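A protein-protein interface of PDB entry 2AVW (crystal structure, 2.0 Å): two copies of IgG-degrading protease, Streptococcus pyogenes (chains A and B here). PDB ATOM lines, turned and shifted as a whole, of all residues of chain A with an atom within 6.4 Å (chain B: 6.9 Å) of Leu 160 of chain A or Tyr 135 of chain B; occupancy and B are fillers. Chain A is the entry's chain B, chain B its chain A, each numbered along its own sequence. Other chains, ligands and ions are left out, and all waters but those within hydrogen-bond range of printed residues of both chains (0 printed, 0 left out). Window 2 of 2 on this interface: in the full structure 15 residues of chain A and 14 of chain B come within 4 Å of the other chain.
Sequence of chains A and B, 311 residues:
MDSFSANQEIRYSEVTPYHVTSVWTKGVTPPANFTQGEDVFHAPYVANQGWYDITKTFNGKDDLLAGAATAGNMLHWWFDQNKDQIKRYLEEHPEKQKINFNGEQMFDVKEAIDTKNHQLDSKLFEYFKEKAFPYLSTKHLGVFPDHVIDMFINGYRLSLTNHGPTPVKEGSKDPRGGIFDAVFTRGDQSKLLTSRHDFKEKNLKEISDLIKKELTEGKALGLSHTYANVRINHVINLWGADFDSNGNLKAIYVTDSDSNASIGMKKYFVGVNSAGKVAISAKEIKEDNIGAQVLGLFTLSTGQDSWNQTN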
ATOM      1  N   ALA A 132       7.731 -10.552  26.095  1.00  0.00           N
ATOM      2  CA  ALA A 132       8.115 -11.102  24.799  1.00  0.00           C
ATOM      3  C   ALA A 132       7.656 -12.531  24.529  1.00  0.00           C
ATOM      4  O   ALA A 132       7.071 -12.813  23.483  1.00  0.00           O
ATOM      5  CB  ALA A 132       9.626 -11.016  24.636  1.00  0.00           C
ATOM      6  N   PHE A 133       7.928 -13.433  25.466  1.00  0.00           N
ATOM      7  CA  PHE A 133       7.565 -14.835  25.292  1.00  0.00           C
ATOM      8  C   PHE A 133       6.779 -15.372  26.494  1.00  0.00           C
ATOM      9  O   PHE A 133       7.148 -16.379  27.091  1.00  0.00           O
ATOM     10  CB  PHE A 133       8.843 -15.654  25.093  1.00  0.00           C
ATOM     11  CG  PHE A 133       9.840 -15.007  24.168  1.00  0.00           C
ATOM     12  CD1 PHE A 133       9.539 -14.813  22.821  1.00  0.00           C
ATOM     13  CD2 PHE A 133      11.070 -14.571  24.645  1.00  0.00           C
ATOM     14  CE1 PHE A 133      10.455 -14.190  21.966  1.00  0.00           C
ATOM     15  CE2 PHE A 133      11.987 -13.949  23.802  1.00  0.00           C
ATOM     16  CZ  PHE A 133      11.682 -13.758  22.463  1.00  0.00           C
ATOM     17  N   PRO A 134       5.670 -14.713  26.853  1.00  0.00           N
ATOM     18  CA  PRO A 134       4.864 -15.155  27.997  1.00  0.00           C
ATOM     19  C   PRO A 134       4.218 -16.537  27.860  1.00  0.00           C
ATOM     20  O   PRO A 134       4.254 -17.330  28.795  1.00  0.00           O
ATOM     21  CB  PRO A 134       3.803 -14.058  28.124  1.00  0.00           C
ATOM     22  CG  PRO A 134       4.416 -12.873  27.433  1.00  0.00           C
ATOM     23  CD  PRO A 134       5.097 -13.497  26.254  1.00  0.00           C
ATOM     24  N   TYR A 135       3.642 -16.815  26.690  1.00  0.00           N
ATOM     25  CA  TYR A 135       2.929 -18.071  26.444  1.00  0.00           C
ATOM     26  C   TYR A 135       3.708 -19.312  25.997  1.00  0.00           C
ATOM     27  O   TYR A 135       3.160 -20.413  26.018  1.00  0.00           O
ATOM     28  CB  TYR A 135       1.803 -17.819  25.434  1.00  0.00           C
ATOM     29  CG  TYR A 135       0.783 -16.783  25.866  1.00  0.00           C
ATOM     30  CD1 TYR A 135      -0.211 -16.352  24.987  1.00  0.00           C
ATOM     31  CD2 TYR A 135       0.819 -16.223  27.145  1.00  0.00           C
ATOM     32  CE1 TYR A 135      -1.140 -15.386  25.368  1.00  0.00           C
ATOM     33  CE2 TYR A 135      -0.103 -15.258  27.535  1.00  0.00           C
ATOM     34  CZ  TYR A 135      -1.077 -14.842  26.643  1.00  0.00           C
ATOM     35  OH  TYR A 135      -1.980 -13.874  27.026  1.00  0.00           O
ATOM     36  N   LEU A 136       4.964 -19.152  25.593  1.00  0.00           N
ATOM     37  CA  LEU A 136       5.753 -20.298  25.136  1.00  0.00           C
ATOM     38  C   LEU A 136       5.849 -21.466  26.117  1.00  0.00           C
ATOM     39  O   LEU A 136       5.720 -22.623  25.714  1.00  0.00           O
ATOM     40  CB  LEU A 136       7.167 -19.861  24.748  1.00  0.00           C
ATOM     41  CG  LEU A 136       7.264 -19.015  23.480  1.00  0.00           C
ATOM     42  CD1 LEU A 136       8.722 -18.726  23.185  1.00  0.00           C
ATOM     43  CD2 LEU A 136       6.616 -19.746  22.309  1.00  0.00           C
ATOM     44  N   LYS A 139       2.824 -23.604  26.188  1.00  0.00           N
ATOM     45  CA  LYS A 139       2.594 -24.341  24.947  1.00  0.00           C
ATOM     46  C   LYS A 139       3.670 -25.398  24.720  1.00  0.00           C
ATOM     47  O   LYS A 139       3.798 -25.939  23.621  1.00  0.00           O
ATOM     48  CB  LYS A 139       2.579 -23.372  23.765  1.00  0.00           C
ATOM     49  CG  LYS A 139       1.678 -22.173  23.974  1.00  0.00           C
ATOM     50  CD  LYS A 139       1.762 -21.182  22.819  1.00  0.00           C
ATOM     51  CE  LYS A 139       1.245 -21.784  21.523  1.00  0.00           C
ATOM     52  NZ  LYS A 139       1.238 -20.792  20.414  1.00  0.00           N
ATOM     53  N   LEU A 141       6.676 -25.007  24.367  1.00  0.00           N
ATOM     54  CA  LEU A 141       7.613 -24.511  23.365  1.00  0.00           C
ATOM     55  C   LEU A 141       8.744 -23.704  23.999  1.00  0.00           C
ATOM     56  O   LEU A 141       8.535 -22.958  24.958  1.00  0.00           O
ATOM     57  CB  LEU A 141       6.892 -23.617  22.346  1.00  0.00           C
ATOM     58  CG  LEU A 141       5.792 -24.174  21.431  1.00  0.00           C
ATOM     59  CD1 LEU A 141       5.099 -23.017  20.720  1.00  0.00           C
ATOM     60  CD2 LEU A 141       6.381 -25.144  20.420  1.00  0.00           C
ATOM     61  N   GLY A 142       9.943 -23.866  23.452  1.00  0.00           N
ATOM     62  CA  GLY A 142      11.091 -23.116  23.921  1.00  0.00           C
ATOM     63  C   GLY A 142      11.500 -22.188  22.786  1.00  0.00           C
ATOM     64  O   GLY A 142      10.775 -22.071  21.795  1.00  0.00           O
ATOM     65  N   VAL A 143      12.641 -21.519  22.918  1.00  0.00           N
ATOM     66  CA  VAL A 143      13.111 -20.625  21.863  1.00  0.00           C
ATOM     67  C   VAL A 143      14.611 -20.805  21.694  1.00  0.00           C
ATOM     68  O   VAL A 143      15.303 -21.200  22.629  1.00  0.00           O
ATOM     69  CB  VAL A 143      12.848 -19.133  22.187  1.00  0.00           C
ATOM     70  CG1 VAL A 143      12.286 -18.434  20.966  1.00  0.00           C
ATOM     71  CG2 VAL A 143      11.926 -18.997  23.370  1.00  0.00           C
ATOM     72  N   LEU A 158      10.232 -12.936  15.016  1.00  0.00           N
ATOM     73  CA  LEU A 158      10.447 -14.281  15.507  1.00  0.00           C
ATOM     74  C   LEU A 158       9.165 -15.079  15.330  1.00  0.00           C
ATOM     75  O   LEU A 158       8.109 -14.700  15.839  1.00  0.00           O
ATOM     76  CB  LEU A 158      10.857 -14.235  16.983  1.00  0.00           C
ATOM     77  CG  LEU A 158      11.435 -15.500  17.622  1.00  0.00           C
ATOM     78  CD1 LEU A 158      12.071 -15.130  18.947  1.00  0.00           C
ATOM     79  CD2 LEU A 158      10.352 -16.555  17.816  1.00  0.00           C
ATOM     80  N   SER A 159       9.254 -16.171  14.579  1.00  0.00           N
ATOM     81  CA  SER A 159       8.101 -17.026  14.354  1.00  0.00           C
ATOM     82  C   SER A 159       8.410 -18.353  15.030  1.00  0.00           C
ATOM     83  O   SER A 159       9.510 -18.888  14.891  1.00  0.00           O
ATOM     84  CB  SER A 159       7.858 -17.226  12.859  1.00  0.00           C
ATOM     85  OG  SER A 159       6.524 -17.649  12.624  1.00  0.00           O
ATOM     86  N   LEU A 160       7.436 -18.875  15.767  1.00  0.00           N
ATOM     87  CA  LEU A 160       7.606 -20.120  16.507  1.00  0.00           C
ATOM     88  C   LEU A 160       7.649 -21.388  15.652  1.00  0.00           C
ATOM     89  O   LEU A 160       7.985 -22.466  16.147  1.00  0.00           O
ATOM     90  CB  LEU A 160       6.496 -20.230  17.555  1.00  0.00           C
ATOM     91  CG  LEU A 160       6.392 -19.002  18.468  1.00  0.00           C
ATOM     92  CD1 LEU A 160       5.170 -19.117  19.364  1.00  0.00           C
ATOM     93  CD2 LEU A 160       7.663 -18.869  19.294  1.00  0.00           C
ATOM     94  N   THR A 161       7.318 -21.260  14.372  1.00  0.00           N
ATOM     95  CA  THR A 161       7.326 -22.411  13.476  1.00  0.00           C
ATOM     96  C   THR A 161       8.623 -22.511  12.674  1.00  0.00           C
ATOM     97  O   THR A 161       8.838 -23.482  11.945  1.00  0.00           O
ATOM     98  CB  THR A 161       6.137 -22.353  12.504  1.00  0.00           C
ATOM     99  OG1 THR A 161       6.161 -21.109  11.792  1.00  0.00           O
ATOM    100  CG2 THR A 161       4.828 -22.471  13.265  1.00  0.00           C
ATOM    101  N   ASN A 162       9.484 -21.507  12.819  1.00  0.00           N
ATOM    102  CA  ASN A 162      10.763 -21.471  12.115  1.00  0.00           C
ATOM    103  C   ASN A 162      11.783 -22.413  12.765  1.00  0.00           C
ATOM    104  O   ASN A 162      12.562 -21.997  13.626  1.00  0.00           O
ATOM    105  CB  ASN A 162      11.313 -20.040  12.116  1.00  0.00           C
ATOM    106  CG  ASN A 162      12.576 -19.897  11.290  1.00  0.00           C
ATOM    107  OD1 ASN A 162      13.271 -18.882  11.369  1.00  0.00           O
ATOM    108  ND2 ASN A 162      12.877 -20.910  10.484  1.00  0.00           N
ATOM    109  N   HIS A 163      11.777 -23.678  12.351  1.00  0.00           N
ATOM    110  CA  HIS A 163      12.704 -24.667  12.901  1.00  0.00           C
ATOM    111  C   HIS A 163      14.140 -24.458  12.429  1.00  0.00           C
ATOM    112  O   HIS A 163      15.064 -25.095  12.938  1.00  0.00           O
ATOM    113  CB  HIS A 163      12.260 -26.087  12.528  1.00  0.00           C
ATOM    114  CG  HIS A 163      11.305 -26.704  13.503  1.00  0.00           C
ATOM    115  ND1 HIS A 163      10.062 -26.170  13.768  1.00  0.00           N
ATOM    116  CD2 HIS A 163      11.414 -27.808  14.280  1.00  0.00           C
ATOM    117  CE1 HIS A 163       9.448 -26.918  14.667  1.00  0.00           C
ATOM    118  NE2 HIS A 163      10.245 -27.917  14.995  1.00  0.00           N
ATOM    119  N   ARG A 176       8.391  -6.444  19.291  1.00  0.00           N
ATOM    120  CA  ARG A 176       9.103  -6.815  20.505  1.00  0.00           C
ATOM    121  C   ARG A 176      10.598  -6.524  20.470  1.00  0.00           C
ATOM    122  O   ARG A 176      11.258  -6.615  21.498  1.00  0.00           O
ATOM    123  CB  ARG A 176       8.904  -8.301  20.797  1.00  0.00           C
ATOM    124  CG  ARG A 176       7.471  -8.682  21.111  1.00  0.00           C
ATOM    125  CD  ARG A 176       7.297 -10.187  21.108  1.00  0.00           C
ATOM    126  NE  ARG A 176       7.565 -10.740  19.785  1.00  0.00           N
ATOM    127  CZ  ARG A 176       7.392 -12.014  19.457  1.00  0.00           C
ATOM    128  NH1 ARG A 176       6.951 -12.878  20.366  1.00  0.00           N
ATOM    129  NH2 ARG A 176       7.636 -12.417  18.215  1.00  0.00           N
ATOM    130  N   LYS B  61      -5.432 -19.233  12.835  1.00  0.00           N
ATOM    131  CA  LYS B  61      -5.438 -18.277  13.933  1.00  0.00           C
ATOM    132  C   LYS B  61      -6.804 -18.113  14.600  1.00  0.00           C
ATOM    133  O   LYS B  61      -6.881 -17.976  15.816  1.00  0.00           O
ATOM    134  CB  LYS B  61      -4.917 -16.924  13.437  1.00  0.00           C
ATOM    135  CG  LYS B  61      -3.456 -16.993  13.003  1.00  0.00           C
ATOM    136  CD  LYS B  61      -2.892 -15.642  12.610  1.00  0.00           C
ATOM    137  CE  LYS B  61      -1.461 -15.778  12.084  1.00  0.00           C
ATOM    138  NZ  LYS B  61      -0.872 -14.454  11.724  1.00  0.00           N
ATOM    139  N   LYS B 129      -7.918 -12.071  15.940  1.00  0.00           N
ATOM    140  CA  LYS B 129      -7.237 -13.288  15.499  1.00  0.00           C
ATOM    141  C   LYS B 129      -5.766 -13.097  15.178  1.00  0.00           C
ATOM    142  O   LYS B 129      -4.956 -13.984  15.442  1.00  0.00           O
ATOM    143  CB  LYS B 129      -7.945 -13.898  14.276  1.00  0.00           C
ATOM    144  CG  LYS B 129      -7.669 -13.184  12.963  1.00  0.00           C
ATOM    145  CD  LYS B 129      -8.323 -13.896  11.775  1.00  0.00           C
ATOM    146  CE  LYS B 129      -9.828 -13.682  11.727  1.00  0.00           C
ATOM    147  NZ  LYS B 129     -10.426 -14.311  10.503  1.00  0.00           N
ATOM    148  N   GLU B 130      -5.419 -11.937  14.630  1.00  0.00           N
ATOM    149  CA  GLU B 130      -4.041 -11.656  14.228  1.00  0.00           C
ATOM    150  C   GLU B 130      -3.128 -11.038  15.279  1.00  0.00           C
ATOM    151  O   GLU B 130      -1.950 -11.380  15.341  1.00  0.00           O
ATOM    152  CB  GLU B 130      -4.027 -10.744  12.994  1.00  0.00           C
ATOM    153  CG  GLU B 130      -4.750 -11.297  11.784  1.00  0.00           C
ATOM    154  CD  GLU B 130      -4.074 -12.520  11.201  1.00  0.00           C
ATOM    155  OE1 GLU B 130      -4.687 -13.176  10.329  1.00  0.00           O
ATOM    156  OE2 GLU B 130      -2.931 -12.825  11.609  1.00  0.00           O
ATOM    157  N   LYS B 131      -3.650 -10.134  16.105  1.00  0.00           N
ATOM    158  CA  LYS B 131      -2.801  -9.464  17.094  1.00  0.00           C
ATOM    159  C   LYS B 131      -3.117  -9.690  18.567  1.00  0.00           C
ATOM    160  O   LYS B 131      -2.207  -9.851  19.381  1.00  0.00           O
ATOM    161  CB  LYS B 131      -2.808  -7.956  16.831  1.00  0.00           C
ATOM    162  CG  LYS B 131      -2.527  -7.551  15.397  1.00  0.00           C
ATOM    163  CD  LYS B 131      -1.111  -7.910  14.985  1.00  0.00           C
ATOM    164  CE  LYS B 131      -0.781  -7.358  13.607  1.00  0.00           C
ATOM    165  NZ  LYS B 131       0.633  -7.658  13.215  1.00  0.00           N
ATOM    166  N   ALA B 132      -4.400  -9.698  18.920  1.00  0.00           N
ATOM    167  CA  ALA B 132      -4.789  -9.864  20.322  1.00  0.00           C
ATOM    168  C   ALA B 132      -4.734 -11.285  20.886  1.00  0.00           C
ATOM    169  O   ALA B 132      -4.232 -11.491  21.988  1.00  0.00           O
ATOM    170  CB  ALA B 132      -6.193  -9.273  20.546  1.00  0.00           C
ATOM    171  N   PHE B 133      -5.254 -12.262  20.147  1.00  0.00           N
ATOM    172  CA  PHE B 133      -5.265 -13.637  20.638  1.00  0.00           C
ATOM    173  C   PHE B 133      -4.783 -14.656  19.602  1.00  0.00           C
ATOM    174  O   PHE B 133      -5.419 -15.691  19.408  1.00  0.00           O
ATOM    175  CB  PHE B 133      -6.686 -14.015  21.067  1.00  0.00           C
ATOM    176  CG  PHE B 133      -7.396 -12.941  21.839  1.00  0.00           C
ATOM    177  CD1 PHE B 133      -6.918 -12.516  23.071  1.00  0.00           C
ATOM    178  CD2 PHE B 133      -8.553 -12.353  21.326  1.00  0.00           C
ATOM    179  CE1 PHE B 133      -7.578 -11.523  23.785  1.00  0.00           C
ATOM    180  CE2 PHE B 133      -9.218 -11.358  22.032  1.00  0.00           C
ATOM    181  CZ  PHE B 133      -8.727 -10.942  23.266  1.00  0.00           C
ATOM    182  N   PRO B 134      -3.648 -14.392  18.937  1.00  0.00           N
ATOM    183  CA  PRO B 134      -3.156 -15.342  17.931  1.00  0.00           C
ATOM    184  C   PRO B 134      -2.797 -16.711  18.509  1.00  0.00           C
ATOM    185  O   PRO B 134      -3.261 -17.744  18.021  1.00  0.00           O
ATOM    186  CB  PRO B 134      -1.930 -14.637  17.350  1.00  0.00           C
ATOM    187  CG  PRO B 134      -2.149 -13.182  17.690  1.00  0.00           C
ATOM    188  CD  PRO B 134      -2.726 -13.254  19.070  1.00  0.00           C
ATOM    189  N   TYR B 135      -1.974 -16.702  19.555  1.00  0.00           N
ATOM    190  CA  TYR B 135      -1.503 -17.923  20.213  1.00  0.00           C
ATOM    191  C   TYR B 135      -2.563 -18.913  20.700  1.00  0.00           C
ATOM    192  O   TYR B 135      -2.335 -20.122  20.680  1.00  0.00           O
ATOM    193  CB  TYR B 135      -0.604 -17.572  21.408  1.00  0.00           C
ATOM    194  CG  TYR B 135       0.750 -16.983  21.059  1.00  0.00           C
ATOM    195  CD1 TYR B 135       1.870 -17.276  21.840  1.00  0.00           C
ATOM    196  CD2 TYR B 135       0.912 -16.122  19.972  1.00  0.00           C
ATOM    197  CE1 TYR B 135       3.115 -16.730  21.548  1.00  0.00           C
ATOM    198  CE2 TYR B 135       2.158 -15.567  19.672  1.00  0.00           C
ATOM    199  CZ  TYR B 135       3.254 -15.878  20.467  1.00  0.00           C
ATOM    200  OH  TYR B 135       4.488 -15.337  20.186  1.00  0.00           O
ATOM    201  N   LEU B 136      -3.704 -18.402  21.149  1.00  0.00           N
ATOM    202  CA  LEU B 136      -4.781 -19.240  21.672  1.00  0.00           C
ATOM    203  C   LEU B 136      -5.206 -20.451  20.840  1.00  0.00           C
ATOM    204  O   LEU B 136      -5.477 -21.515  21.398  1.00  0.00           O
ATOM    205  CB  LEU B 136      -6.003 -18.373  21.969  1.00  0.00           C
ATOM    206  CG  LEU B 136      -5.760 -17.395  23.118  1.00  0.00           C
ATOM    207  CD1 LEU B 136      -6.886 -16.395  23.185  1.00  0.00           C
ATOM    208  CD2 LEU B 136      -5.637 -18.168  24.423  1.00  0.00           C
ATOM    209  N   SER B 137      -5.273 -20.300  19.519  1.00  0.00           N
ATOM    210  CA  SER B 137      -5.678 -21.411  18.662  1.00  0.00           C
ATOM    211  C   SER B 137      -4.601 -22.492  18.538  1.00  0.00           C
ATOM    212  O   SER B 137      -4.837 -23.553  17.953  1.00  0.00           O
ATOM    213  CB  SER B 137      -6.074 -20.897  17.271  1.00  0.00           C
ATOM    214  OG  SER B 137      -7.280 -20.150  17.329  1.00  0.00           O
ATOM    215  N   THR B 138      -3.424 -22.219  19.093  1.00  0.00           N
ATOM    216  CA  THR B 138      -2.314 -23.168  19.066  1.00  0.00           C
ATOM    217  C   THR B 138      -2.106 -23.742  20.470  1.00  0.00           C
ATOM    218  O   THR B 138      -1.221 -24.571  20.695  1.00  0.00           O
ATOM    219  CB  THR B 138      -1.005 -22.486  18.591  1.00  0.00           C
ATOM    220  OG1 THR B 138      -1.199 -21.950  17.276  1.00  0.00           O
ATOM    221  CG2 THR B 138       0.143 -23.484  18.546  1.00  0.00           C
ATOM    222  N   LYS B 139      -2.939 -23.295  21.408  1.00  0.00           N
ATOM    223  CA  LYS B 139      -2.873 -23.748  22.796  1.00  0.00           C
ATOM    224  C   LYS B 139      -4.160 -24.458  23.194  1.00  0.00           C
ATOM    225  O   LYS B 139      -4.380 -24.746  24.373  1.00  0.00           O
ATOM    226  CB  LYS B 139      -2.654 -22.562  23.733  1.00  0.00           C
ATOM    227  CG  LYS B 139      -1.438 -21.720  23.401  1.00  0.00           C
ATOM    228  CD  LYS B 139      -1.237 -20.611  24.426  1.00  0.00           C
ATOM    229  CE  LYS B 139      -1.005 -21.179  25.819  1.00  0.00           C
ATOM    230  NZ  LYS B 139      -0.858 -20.110  26.843  1.00  0.00           N
ATOM    231  N   HIS B 140      -5.008 -24.731  22.205  1.00  0.00           N
ATOM    232  CA  HIS B 140      -6.282 -25.403  22.439  1.00  0.00           C
ATOM    233  C   HIS B 140      -7.065 -24.613  23.483  1.00  0.00           C
ATOM    234  O   HIS B 140      -7.908 -25.162  24.195  1.00  0.00           O
ATOM    235  CB  HIS B 140      -6.039 -26.831  22.937  1.00  0.00           C
ATOM    236  CG  HIS B 140      -4.832 -27.482  22.334  1.00  0.00           C
ATOM    237  ND1 HIS B 140      -4.652 -27.603  20.972  1.00  0.00           N
ATOM    238  CD2 HIS B 140      -3.732 -28.027  22.908  1.00  0.00           C
ATOM    239  CE1 HIS B 140      -3.494 -28.193  20.734  1.00  0.00           C
ATOM    240  NE2 HIS B 140      -2.916 -28.461  21.892  1.00  0.00           N
ATOM    241  N   LEU B 141      -6.775 -23.320  23.561  1.00  0.00           N
ATOM    242  CA  LEU B 141      -7.432 -22.446  24.521  1.00  0.00           C
ATOM    243  C   LEU B 141      -8.383 -21.460  23.863  1.00  0.00           C
ATOM    244  O   LEU B 141      -8.108 -20.923  22.787  1.00  0.00           O
ATOM    245  CB  LEU B 141      -6.389 -21.671  25.330  1.00  0.00           C
ATOM    246  CG  LEU B 141      -5.461 -22.445  26.270  1.00  0.00           C
ATOM    247  CD1 LEU B 141      -4.427 -21.492  26.852  1.00  0.00           C
ATOM    248  CD2 LEU B 141      -6.274 -23.100  27.383  1.00  0.00           C
ATOM    249  N   LEU B 160      -5.951 -15.672  30.832  1.00  0.00           N
ATOM    250  CA  LEU B 160      -6.345 -16.938  30.220  1.00  0.00           C
ATOM    251  C   LEU B 160      -6.677 -18.007  31.257  1.00  0.00           C
ATOM    252  O   LEU B 160      -7.410 -18.954  30.966  1.00  0.00           O
ATOM    253  CB  LEU B 160      -5.232 -17.446  29.301  1.00  0.00           C
ATOM    254  CG  LEU B 160      -4.813 -16.513  28.161  1.00  0.00           C
ATOM    255  CD1 LEU B 160      -3.711 -17.169  27.341  1.00  0.00           C
ATOM    256  CD2 LEU B 160      -6.017 -16.195  27.287  1.00  0.00           C
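The guanidinium group of Arg 176 of chain A lies within hydrogen-bond range of the side-chain hydroxyl of Tyr 135 of chain B, at 3.5 Å.
O of Ala 132 of chain A sits at hydrogen-bond distance from NH1 of Arg 176 of chain A (3.1 Å). O of Leu 158 of chain A sits at hydrogen-bond distance from NH2 of Arg 176 of chain A, at 3.3 Å.
CD1 of Tyr 135 of chain B touches CB of Tyr 135 of chain A, 3.6 Å away. NZ of Lys 139 of chain B touches CB of Tyr 135 of chain A (3.8 Å). Tyr 135 of chain A touches Leu 160 of chain B. Lys 139 of chain A touches Tyr 135 of chain B (NZ to O, 3.6 Å). NZ of Lys 139 of chain A touches CB of Thr 138 of chain B, 3.4 Å away. CG of Lys 139 of chain A touches CG of Lys 139 of chain B (3.2 Å). Leu 160 of chain A touches Tyr 135 of chain B (CD1 to CE1, 3.8 Å).
Of the printed residues of chain B, Tyr 135 of chain A touches Tyr 135, Lys 139 and Leu 160. Leu 160 of chain A touches one residue of chain B. Ala 132 of chain B touches none of the printed residues of chain A. Of the printed residues of chain A, Tyr 135 of chain B touches Tyr 135 (3.6 Å), Lys 139 (3.6 Å), Leu 160 (3.8 Å) and Arg 176 (3.5 Å). Of the printed residues of chain A, Leu 160 of chain B touches Tyr 135. The nearest residue of chain B that does not touch Leu 160 of chain A is Thr 138 of chain B (6.7 Å). The nearest residue of chain A that does not touch Tyr 135 of chain B is Leu 136 of chain A (4.7 Å). The nearest printed residue of chain A that does not touch Thr 138 of chain B is Leu 141 of chain A (5.4 Å).
Of the 16 printed residues of chain A, 4 touch a printed residue of chain B. Hydrophobic or aromatic side chains of chain A that line the printed part of chain B: Tyr 135 and Leu 160. Along chain A the printed residues that touch a printed residue of chain B span positions 135 to 176. Hydrophobic or aromatic side chains of chain B that line the printed part of chain A: Tyr 135 and Leu 160. Along chain B the printed residues that touch a printed residue of chain A span positions 135 to 160. Among the printed residues, 8 pairs touch across the chains. Among the printed residues, no Asp or Glu carboxylate lies within 4 Å of a Lys or Arg side-chain nitrogen of the other chain.
Tyr 135 of chain A touches its own counterpart, Tyr 135 of chain B. Tyr 135 of chain A touches Lys 139 of chain B, and with the chains exchanged Lys 139 of chain A touches Tyr 135 of chain B. Tyr 135 of chain A touches Leu 160 of chain B, and with the chains exchanged Leu 160 of chain A touches Tyr 135 of chain B. Lys 139 of chain A touches its own counterpart, Lys 139 of chain B. Positions printed for both chains: 132, 133, 134, 135, 136, 139, 141 and 160. Of the 8 pairs that touch across the chains among the printed residues, 6 have their exchanged pair printed and touching as well.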
